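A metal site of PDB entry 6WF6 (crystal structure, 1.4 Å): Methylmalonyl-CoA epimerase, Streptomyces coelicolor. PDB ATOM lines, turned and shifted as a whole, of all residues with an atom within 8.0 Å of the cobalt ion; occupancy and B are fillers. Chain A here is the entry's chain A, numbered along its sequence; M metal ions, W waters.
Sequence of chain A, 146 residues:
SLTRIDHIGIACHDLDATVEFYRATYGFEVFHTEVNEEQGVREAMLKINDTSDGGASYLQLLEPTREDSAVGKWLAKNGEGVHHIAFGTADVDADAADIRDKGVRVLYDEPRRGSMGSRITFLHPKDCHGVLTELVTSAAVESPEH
Four residues have an atom within 4 Å of the cobalt ion: His 7, Gln 60, His 84 and Glu 134.
Along chain A the residues within 4 Å of the cobalt ion span positions 7 to 134.
The cobalt ion is bound by the side-chain carboxylate of Glu 134 (2.0 Å), a ring nitrogen (NE2) of His 84 (2.1 Å), water W2 (2.2 Å), a ring nitrogen (NE2) of His 7 (2.2 Å), the side-chain amide oxygen of Gln 60 (2.2 Å) and water W1 (2.6 Å).
The backbone NH of Glu 134 is in hydrogen-bond range of the backbone carbonyl oxygen of Ile 85 (2.8 Å).
O of Gln 60 is in hydrogen-bond range of N of Ile 10, at 2.8 Å.
The backbone NH of Gln 60 sits at hydrogen-bond distance from the backbone carbonyl oxygen of Ile 8, 2.8 Å away.
The side-chain sulfur (SD) of Met 45 lies close to the side-chain amide nitrogen (NE2) of Gln 60 (3.6 Å).
The side-chain carboxylate (OD2) of Asp 6 is in hydrogen-bond range of a ring nitrogen (ND1) of His 7.
The backbone NH (N) of Gly 9 sits at hydrogen-bond distance from the backbone carbonyl oxygen (O) of His 84.
O of His 7 sits at hydrogen-bond distance from N of Ala 86, 2.9 Å away.
A ring nitrogen (ND1) of His 84 lies within hydrogen-bond range of a ring nitrogen (ND1) of His 83, at 2.8 Å.
Water W1 bridges OE2 of Glu 134 and NE2 of Gln 60.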
ATOM      1  N   ASP A   6      20.804  16.952  -9.615  1.00  0.00           N
ATOM      2  CA  ASP A   6      19.846  16.399  -8.640  1.00  0.00           C
ATOM      3  C   ASP A   6      20.425  16.390  -7.250  1.00  0.00           C
ATOM      4  O   ASP A   6      19.731  16.875  -6.299  1.00  0.00           O
ATOM      5  CB  ASP A   6      19.372  15.010  -9.004  1.00  0.00           C
ATOM      6  CG  ASP A   6      18.187  14.559  -8.154  1.00  0.00           C
ATOM      7  OD1 ASP A   6      17.035  14.971  -8.516  1.00  0.00           O
ATOM      8  OD2 ASP A   6      18.413  13.879  -7.135  1.00  0.00           O
ATOM      9  N   HIS A   7      21.647  15.919  -7.054  1.00  0.00           N
ATOM     10  CA  HIS A   7      22.205  15.940  -5.683  1.00  0.00           C
ATOM     11  C   HIS A   7      23.696  15.775  -5.731  1.00  0.00           C
ATOM     12  O   HIS A   7      24.254  15.326  -6.762  1.00  0.00           O
ATOM     13  CB  HIS A   7      21.494  14.945  -4.760  1.00  0.00           C
ATOM     14  CG  HIS A   7      21.634  13.488  -5.147  1.00  0.00           C
ATOM     15  ND1 HIS A   7      20.667  12.839  -5.883  1.00  0.00           N
ATOM     16  CD2 HIS A   7      22.534  12.548  -4.784  1.00  0.00           C
ATOM     17  CE1 HIS A   7      21.015  11.536  -5.956  1.00  0.00           C
ATOM     18  NE2 HIS A   7      22.158  11.320  -5.356  1.00  0.00           N
ATOM     19  N   ILE A   8      24.311  16.057  -4.588  1.00  0.00           N
ATOM     20  CA  ILE A   8      25.720  15.733  -4.323  1.00  0.00           C
ATOM     21  C   ILE A   8      25.683  14.657  -3.248  1.00  0.00           C
ATOM     22  O   ILE A   8      25.115  14.938  -2.169  1.00  0.00           O
ATOM     23  CB  ILE A   8      26.476  16.987  -3.869  1.00  0.00           C
ATOM     24  CG1 ILE A   8      26.368  18.131  -4.886  1.00  0.00           C
ATOM     25  CG2 ILE A   8      27.918  16.593  -3.565  1.00  0.00           C
ATOM     26  CD1 ILE A   8      26.758  19.500  -4.370  1.00  0.00           C
ATOM     27  N   GLY A   9      26.313  13.517  -3.476  1.00  0.00           N
ATOM     28  CA  GLY A   9      26.436  12.434  -2.490  1.00  0.00           C
ATOM     29  C   GLY A   9      27.674  12.611  -1.654  1.00  0.00           C
ATOM     30  O   GLY A   9      28.775  12.718  -2.196  1.00  0.00           O
ATOM     31  N   ILE A  10      27.488  12.748  -0.358  1.00  0.00           N
ATOM     32  CA  ILE A  10      28.549  13.063   0.631  1.00  0.00           C
ATOM     33  C   ILE A  10      28.586  11.905   1.613  1.00  0.00           C
ATOM     34  O   ILE A  10      27.576  11.656   2.306  1.00  0.00           O
ATOM     35  CB  ILE A  10      28.256  14.416   1.282  1.00  0.00           C
ATOM     36  CG1 ILE A  10      28.292  15.544   0.266  1.00  0.00           C
ATOM     37  CG2 ILE A  10      29.236  14.667   2.421  1.00  0.00           C
ATOM     38  CD1 ILE A  10      27.927  16.865   0.770  1.00  0.00           C
ATOM     39  N   GLN A  39      21.868  -1.352  -0.956  1.00  0.00           N
ATOM     40  CA  GLN A  39      23.140  -0.597  -1.054  1.00  0.00           C
ATOM     41  C   GLN A  39      23.929  -0.630   0.266  1.00  0.00           C
ATOM     42  O   GLN A  39      25.162  -0.436   0.204  1.00  0.00           O
ATOM     43  CB  GLN A  39      22.865   0.863  -1.420  1.00  0.00           C
ATOM     44  CG  GLN A  39      22.659   1.093  -2.912  1.00  0.00           C
ATOM     45  CD  GLN A  39      23.031   2.507  -3.333  1.00  0.00           C
ATOM     46  OE1 GLN A  39      23.187   2.799  -4.531  1.00  0.00           O
ATOM     47  NE2 GLN A  39      23.192   3.398  -2.368  1.00  0.00           N
ATOM     48  N   GLU A  43      20.621   7.143   4.369  1.00  0.00           N
ATOM     49  CA  GLU A  43      20.731   8.412   3.609  1.00  0.00           C
ATOM     50  C   GLU A  43      19.876   9.481   4.284  1.00  0.00           C
ATOM     51  O   GLU A  43      18.766   9.173   4.796  1.00  0.00           O
ATOM     52  CB  GLU A  43      20.182   8.362   2.181  1.00  0.00           C
ATOM     53  CG  GLU A  43      20.619   7.212   1.308  1.00  0.00           C
ATOM     54  CD  GLU A  43      19.905   7.039  -0.044  1.00  0.00           C
ATOM     55  OE1 GLU A  43      18.655   7.219  -0.119  1.00  0.00           O
ATOM     56  OE2 GLU A  43      20.608   6.637  -0.996  1.00  0.00           O
ATOM     57  N   MET A  45      18.512  13.193   2.841  1.00  0.00           N
ATOM     58  CA  MET A  45      18.434  14.240   1.798  1.00  0.00           C
ATOM     59  C   MET A  45      18.156  15.570   2.466  1.00  0.00           C
ATOM     60  O   MET A  45      17.193  15.648   3.252  1.00  0.00           O
ATOM     61  CB  MET A  45      17.315  13.877   0.838  1.00  0.00           C
ATOM     62  CG  MET A  45      17.659  12.674  -0.008  1.00  0.00           C
ATOM     63  SD  MET A  45      18.890  13.012  -1.302  1.00  0.00           S
ATOM     64  CE  MET A  45      17.849  13.161  -2.761  1.00  0.00           C
ATOM     65  N   GLN A  60      22.894  14.728  -0.397  1.00  0.00           N
ATOM     66  CA  GLN A  60      22.544  13.360   0.006  1.00  0.00           C
ATOM     67  C   GLN A  60      23.694  12.887   0.899  1.00  0.00           C
ATOM     68  O   GLN A  60      24.773  12.539   0.394  1.00  0.00           O
ATOM     69  CB  GLN A  60      22.402  12.475  -1.234  1.00  0.00           C
ATOM     70  CG  GLN A  60      21.853  11.098  -0.897  1.00  0.00           C
ATOM     71  CD  GLN A  60      21.778  10.310  -2.180  1.00  0.00           C
ATOM     72  OE1 GLN A  60      22.796   9.964  -2.812  1.00  0.00           O
ATOM     73  NE2 GLN A  60      20.551  10.109  -2.606  1.00  0.00           N
ATOM     74  N   LEU A  61      23.466  12.925   2.205  1.00  0.00           N
ATOM     75  CA  LEU A  61      24.472  12.488   3.211  1.00  0.00           C
ATOM     76  C   LEU A  61      24.287  10.997   3.418  1.00  0.00           C
ATOM     77  O   LEU A  61      23.121  10.537   3.538  1.00  0.00           O
ATOM     78  CB  LEU A  61      24.287  13.272   4.514  1.00  0.00           C
ATOM     79  CG  LEU A  61      25.016  14.607   4.555  1.00  0.00           C
ATOM     80  CD1 LEU A  61      24.640  15.534   3.391  1.00  0.00           C
ATOM     81  CD2 LEU A  61      24.725  15.282   5.893  1.00  0.00           C
ATOM     82  N   LEU A  62      25.344  10.228   3.385  1.00  0.00           N
ATOM     83  CA  LEU A  62      25.275   8.748   3.343  1.00  0.00           C
ATOM     84  C   LEU A  62      26.188   8.207   4.436  1.00  0.00           C
ATOM     85  O   LEU A  62      27.386   8.611   4.426  1.00  0.00           O
ATOM     86  CB  LEU A  62      25.874   8.218   2.023  1.00  0.00           C
ATOM     87  CG  LEU A  62      25.129   8.277   0.694  1.00  0.00           C
ATOM     88  CD1 LEU A  62      23.641   8.323   0.912  1.00  0.00           C
ATOM     89  CD2 LEU A  62      25.698   9.363  -0.199  1.00  0.00           C
ATOM     90  N   HIS A  83      31.350  11.780  -2.496  1.00  0.00           N
ATOM     91  CA  HIS A  83      31.385  10.399  -3.015  1.00  0.00           C
ATOM     92  C   HIS A  83      30.885  10.347  -4.459  1.00  0.00           C
ATOM     93  O   HIS A  83      31.480   9.577  -5.277  1.00  0.00           O
ATOM     94  CB  HIS A  83      30.544   9.501  -2.078  1.00  0.00           C
ATOM     95  CG  HIS A  83      30.361   8.111  -2.547  1.00  0.00           C
ATOM     96  ND1 HIS A  83      29.235   7.693  -3.201  1.00  0.00           N
ATOM     97  CD2 HIS A  83      31.188   7.041  -2.489  1.00  0.00           C
ATOM     98  CE1 HIS A  83      29.361   6.416  -3.517  1.00  0.00           C
ATOM     99  NE2 HIS A  83      30.568   5.986  -3.120  1.00  0.00           N
ATOM    100  N   HIS A  84      29.867  11.123  -4.817  1.00  0.00           N
ATOM    101  CA  HIS A  84      29.338  11.081  -6.200  1.00  0.00           C
ATOM    102  C   HIS A  84      28.548  12.329  -6.493  1.00  0.00           C
ATOM    103  O   HIS A  84      28.206  13.053  -5.548  1.00  0.00           O
ATOM    104  CB  HIS A  84      28.442   9.858  -6.421  1.00  0.00           C
ATOM    105  CG  HIS A  84      27.156   9.746  -5.655  1.00  0.00           C
ATOM    106  ND1 HIS A  84      27.087   9.137  -4.389  1.00  0.00           N
ATOM    107  CD2 HIS A  84      25.878  10.097  -5.926  1.00  0.00           C
ATOM    108  CE1 HIS A  84      25.803   9.124  -3.994  1.00  0.00           C
ATOM    109  NE2 HIS A  84      25.038   9.688  -4.897  1.00  0.00           N
ATOM    110  N   ILE A  85      28.226  12.556  -7.745  1.00  0.00           N
ATOM    111  CA  ILE A  85      27.312  13.633  -8.173  1.00  0.00           C
ATOM    112  C   ILE A  85      26.182  12.992  -8.954  1.00  0.00           C
ATOM    113  O   ILE A  85      26.406  11.953  -9.582  1.00  0.00           O
ATOM    114  CB  ILE A  85      28.040  14.738  -8.948  1.00  0.00           C
ATOM    115  CG1 ILE A  85      28.494  14.283 -10.302  1.00  0.00           C
ATOM    116  CG2 ILE A  85      29.241  15.220  -8.186  1.00  0.00           C
ATOM    117  CD1 ILE A  85      29.175  15.401 -11.109  1.00  0.00           C
ATOM    118  N   ALA A  86      25.036  13.576  -8.929  1.00  0.00           N
ATOM    119  CA  ALA A  86      23.828  13.021  -9.566  1.00  0.00           C
ATOM    120  C   ALA A  86      23.177  14.023 -10.452  1.00  0.00           C
ATOM    121  O   ALA A  86      22.896  15.126  -9.992  1.00  0.00           O
ATOM    122  CB  ALA A  86      22.841  12.478  -8.530  1.00  0.00           C
ATOM    123  N   GLY A 114      16.200   4.139  -5.782  1.00  0.00           N
ATOM    124  CA  GLY A 114      16.985   5.152  -5.051  1.00  0.00           C
ATOM    125  C   GLY A 114      16.119   5.886  -4.048  1.00  0.00           C
ATOM    126  O   GLY A 114      14.929   5.569  -3.959  1.00  0.00           O
ATOM    127  N   SER A 115      16.676   6.972  -3.508  1.00  0.00           N
ATOM    128  CA  SER A 115      16.026   7.842  -2.496  1.00  0.00           C
ATOM    129  C   SER A 115      14.593   8.237  -2.926  1.00  0.00           C
ATOM    130  O   SER A 115      14.402   8.618  -4.096  1.00  0.00           O
ATOM    131  CB  SER A 115      16.913   9.072  -2.345  1.00  0.00           C
ATOM    132  OG  SER A 115      16.253  10.029  -1.561  1.00  0.00           O
ATOM    133  N   SER A 118      12.857   7.026  -6.250  1.00  0.00           N
ATOM    134  CA  SER A 118      13.502   7.317  -7.542  1.00  0.00           C
ATOM    135  C   SER A 118      14.072   6.049  -8.170  1.00  0.00           C
ATOM    136  O   SER A 118      14.094   5.011  -7.538  1.00  0.00           O
ATOM    137  CB  SER A 118      14.581   8.344  -7.344  1.00  0.00           C
ATOM    138  OG  SER A 118      15.617   7.923  -6.480  1.00  0.00           O
ATOM    139  N   ILE A 120      17.496   4.896 -10.389  1.00  0.00           N
ATOM    140  CA  ILE A 120      18.863   5.465 -10.524  1.00  0.00           C
ATOM    141  C   ILE A 120      19.806   4.451 -11.174  1.00  0.00           C
ATOM    142  O   ILE A 120      19.585   3.230 -11.119  1.00  0.00           O
ATOM    143  CB  ILE A 120      19.348   5.960  -9.162  1.00  0.00           C
ATOM    144  CG1 ILE A 120      19.695   4.848  -8.185  1.00  0.00           C
ATOM    145  CG2 ILE A 120      18.308   6.904  -8.548  1.00  0.00           C
ATOM    146  CD1 ILE A 120      20.999   4.099  -8.453  1.00  0.00           C
ATOM    147  N   THR A 121      20.867   4.965 -11.753  1.00  0.00           N
ATOM    148  CA  THR A 121      21.985   4.111 -12.207  1.00  0.00           C
ATOM    149  C   THR A 121      23.278   4.923 -12.081  1.00  0.00           C
ATOM    150  O   THR A 121      23.233   6.120 -11.798  1.00  0.00           O
ATOM    151  CB  THR A 121      21.746   3.607 -13.617  1.00  0.00           C
ATOM    152  OG1 THR A 121      22.699   2.565 -13.834  1.00  0.00           O
ATOM    153  CG2 THR A 121      21.832   4.642 -14.696  1.00  0.00           C
ATOM    154  N   PHE A 122      24.399   4.265 -12.221  1.00  0.00           N
ATOM    155  CA  PHE A 122      25.730   4.878 -12.061  1.00  0.00           C
ATOM    156  C   PHE A 122      26.602   4.617 -13.265  1.00  0.00           C
ATOM    157  O   PHE A 122      26.520   3.553 -13.916  1.00  0.00           O
ATOM    158  CB  PHE A 122      26.460   4.378 -10.818  1.00  0.00           C
ATOM    159  CG  PHE A 122      25.926   4.880  -9.511  1.00  0.00           C
ATOM    160  CD1 PHE A 122      26.426   6.053  -8.982  1.00  0.00           C
ATOM    161  CD2 PHE A 122      24.961   4.149  -8.832  1.00  0.00           C
ATOM    162  CE1 PHE A 122      25.980   6.513  -7.740  1.00  0.00           C
ATOM    163  CE2 PHE A 122      24.493   4.648  -7.620  1.00  0.00           C
ATOM    164  CZ  PHE A 122      25.026   5.807  -7.097  1.00  0.00           C
ATOM    165  N   THR A 133      29.296   9.051 -11.143  1.00  0.00           N
ATOM    166  CA  THR A 133      28.195   9.879 -11.705  1.00  0.00           C
ATOM    167  C   THR A 133      26.915   9.061 -11.664  1.00  0.00           C
ATOM    168  O   THR A 133      26.857   7.977 -12.276  1.00  0.00           O
ATOM    169  CB  THR A 133      28.534  10.402 -13.083  1.00  0.00           C
ATOM    170  OG1 THR A 133      29.757  11.134 -13.017  1.00  0.00           O
ATOM    171  CG2 THR A 133      27.454  11.280 -13.650  1.00  0.00           C
ATOM    172  N   GLU A 134      25.880   9.571 -11.023  1.00  0.00           N
ATOM    173  CA  GLU A 134      24.550   8.947 -10.934  1.00  0.00           C
ATOM    174  C   GLU A 134      23.592   9.653 -11.881  1.00  0.00           C
ATOM    175  O   GLU A 134      23.698  10.904 -12.041  1.00  0.00           O
ATOM    176  CB  GLU A 134      24.051   9.064  -9.493  1.00  0.00           C
ATOM    177  CG  GLU A 134      22.916   8.143  -9.165  1.00  0.00           C
ATOM    178  CD  GLU A 134      22.535   8.182  -7.700  1.00  0.00           C
ATOM    179  OE1 GLU A 134      22.988   9.097  -6.922  1.00  0.00           O
ATOM    180  OE2 GLU A 134      21.622   7.369  -7.370  1.00  0.00           O
ATOM    181  N   LEU A 135      22.724   8.867 -12.512  1.00  0.00           N
ATOM    182  CA  LEU A 135      21.579   9.365 -13.286  1.00  0.00           C
ATOM    183  C   LEU A 135      20.317   9.012 -12.511  1.00  0.00           C
ATOM    184  O   LEU A 135      20.185   7.859 -12.057  1.00  0.00           O
ATOM    185  CB  LEU A 135      21.554   8.774 -14.680  1.00  0.00           C
ATOM    186  CG  LEU A 135      22.877   8.775 -15.446  1.00  0.00           C
ATOM    187  CD1 LEU A 135      22.701   8.099 -16.818  1.00  0.00           C
ATOM    188  CD2 LEU A 135      23.475  10.158 -15.570  1.00  0.00           C
ATOM    189  N   VAL A 136      19.397   9.967 -12.368  1.00  0.00           N
ATOM    190  CA  VAL A 136      18.221   9.900 -11.446  1.00  0.00           C
ATOM    191  C   VAL A 136      16.955  10.312 -12.202  1.00  0.00           C
ATOM    192  O   VAL A 136      16.924  11.428 -12.666  1.00  0.00           O
ATOM    193  CB  VAL A 136      18.395  10.804 -10.201  1.00  0.00           C
ATOM    194  CG1 VAL A 136      17.171  10.809  -9.276  1.00  0.00           C
ATOM    195  CG2 VAL A 136      19.664  10.473  -9.439  1.00  0.00           C
HETATM  196 CO    CO M   1      22.942   9.342  -4.905  1.00  0.00          CO
HETATM  197  O   HOH W   1      20.489   8.559  -5.146  1.00  0.00           O
HETATM  198  O   HOH W   2      23.056   7.304  -4.207  1.00  0.00           O
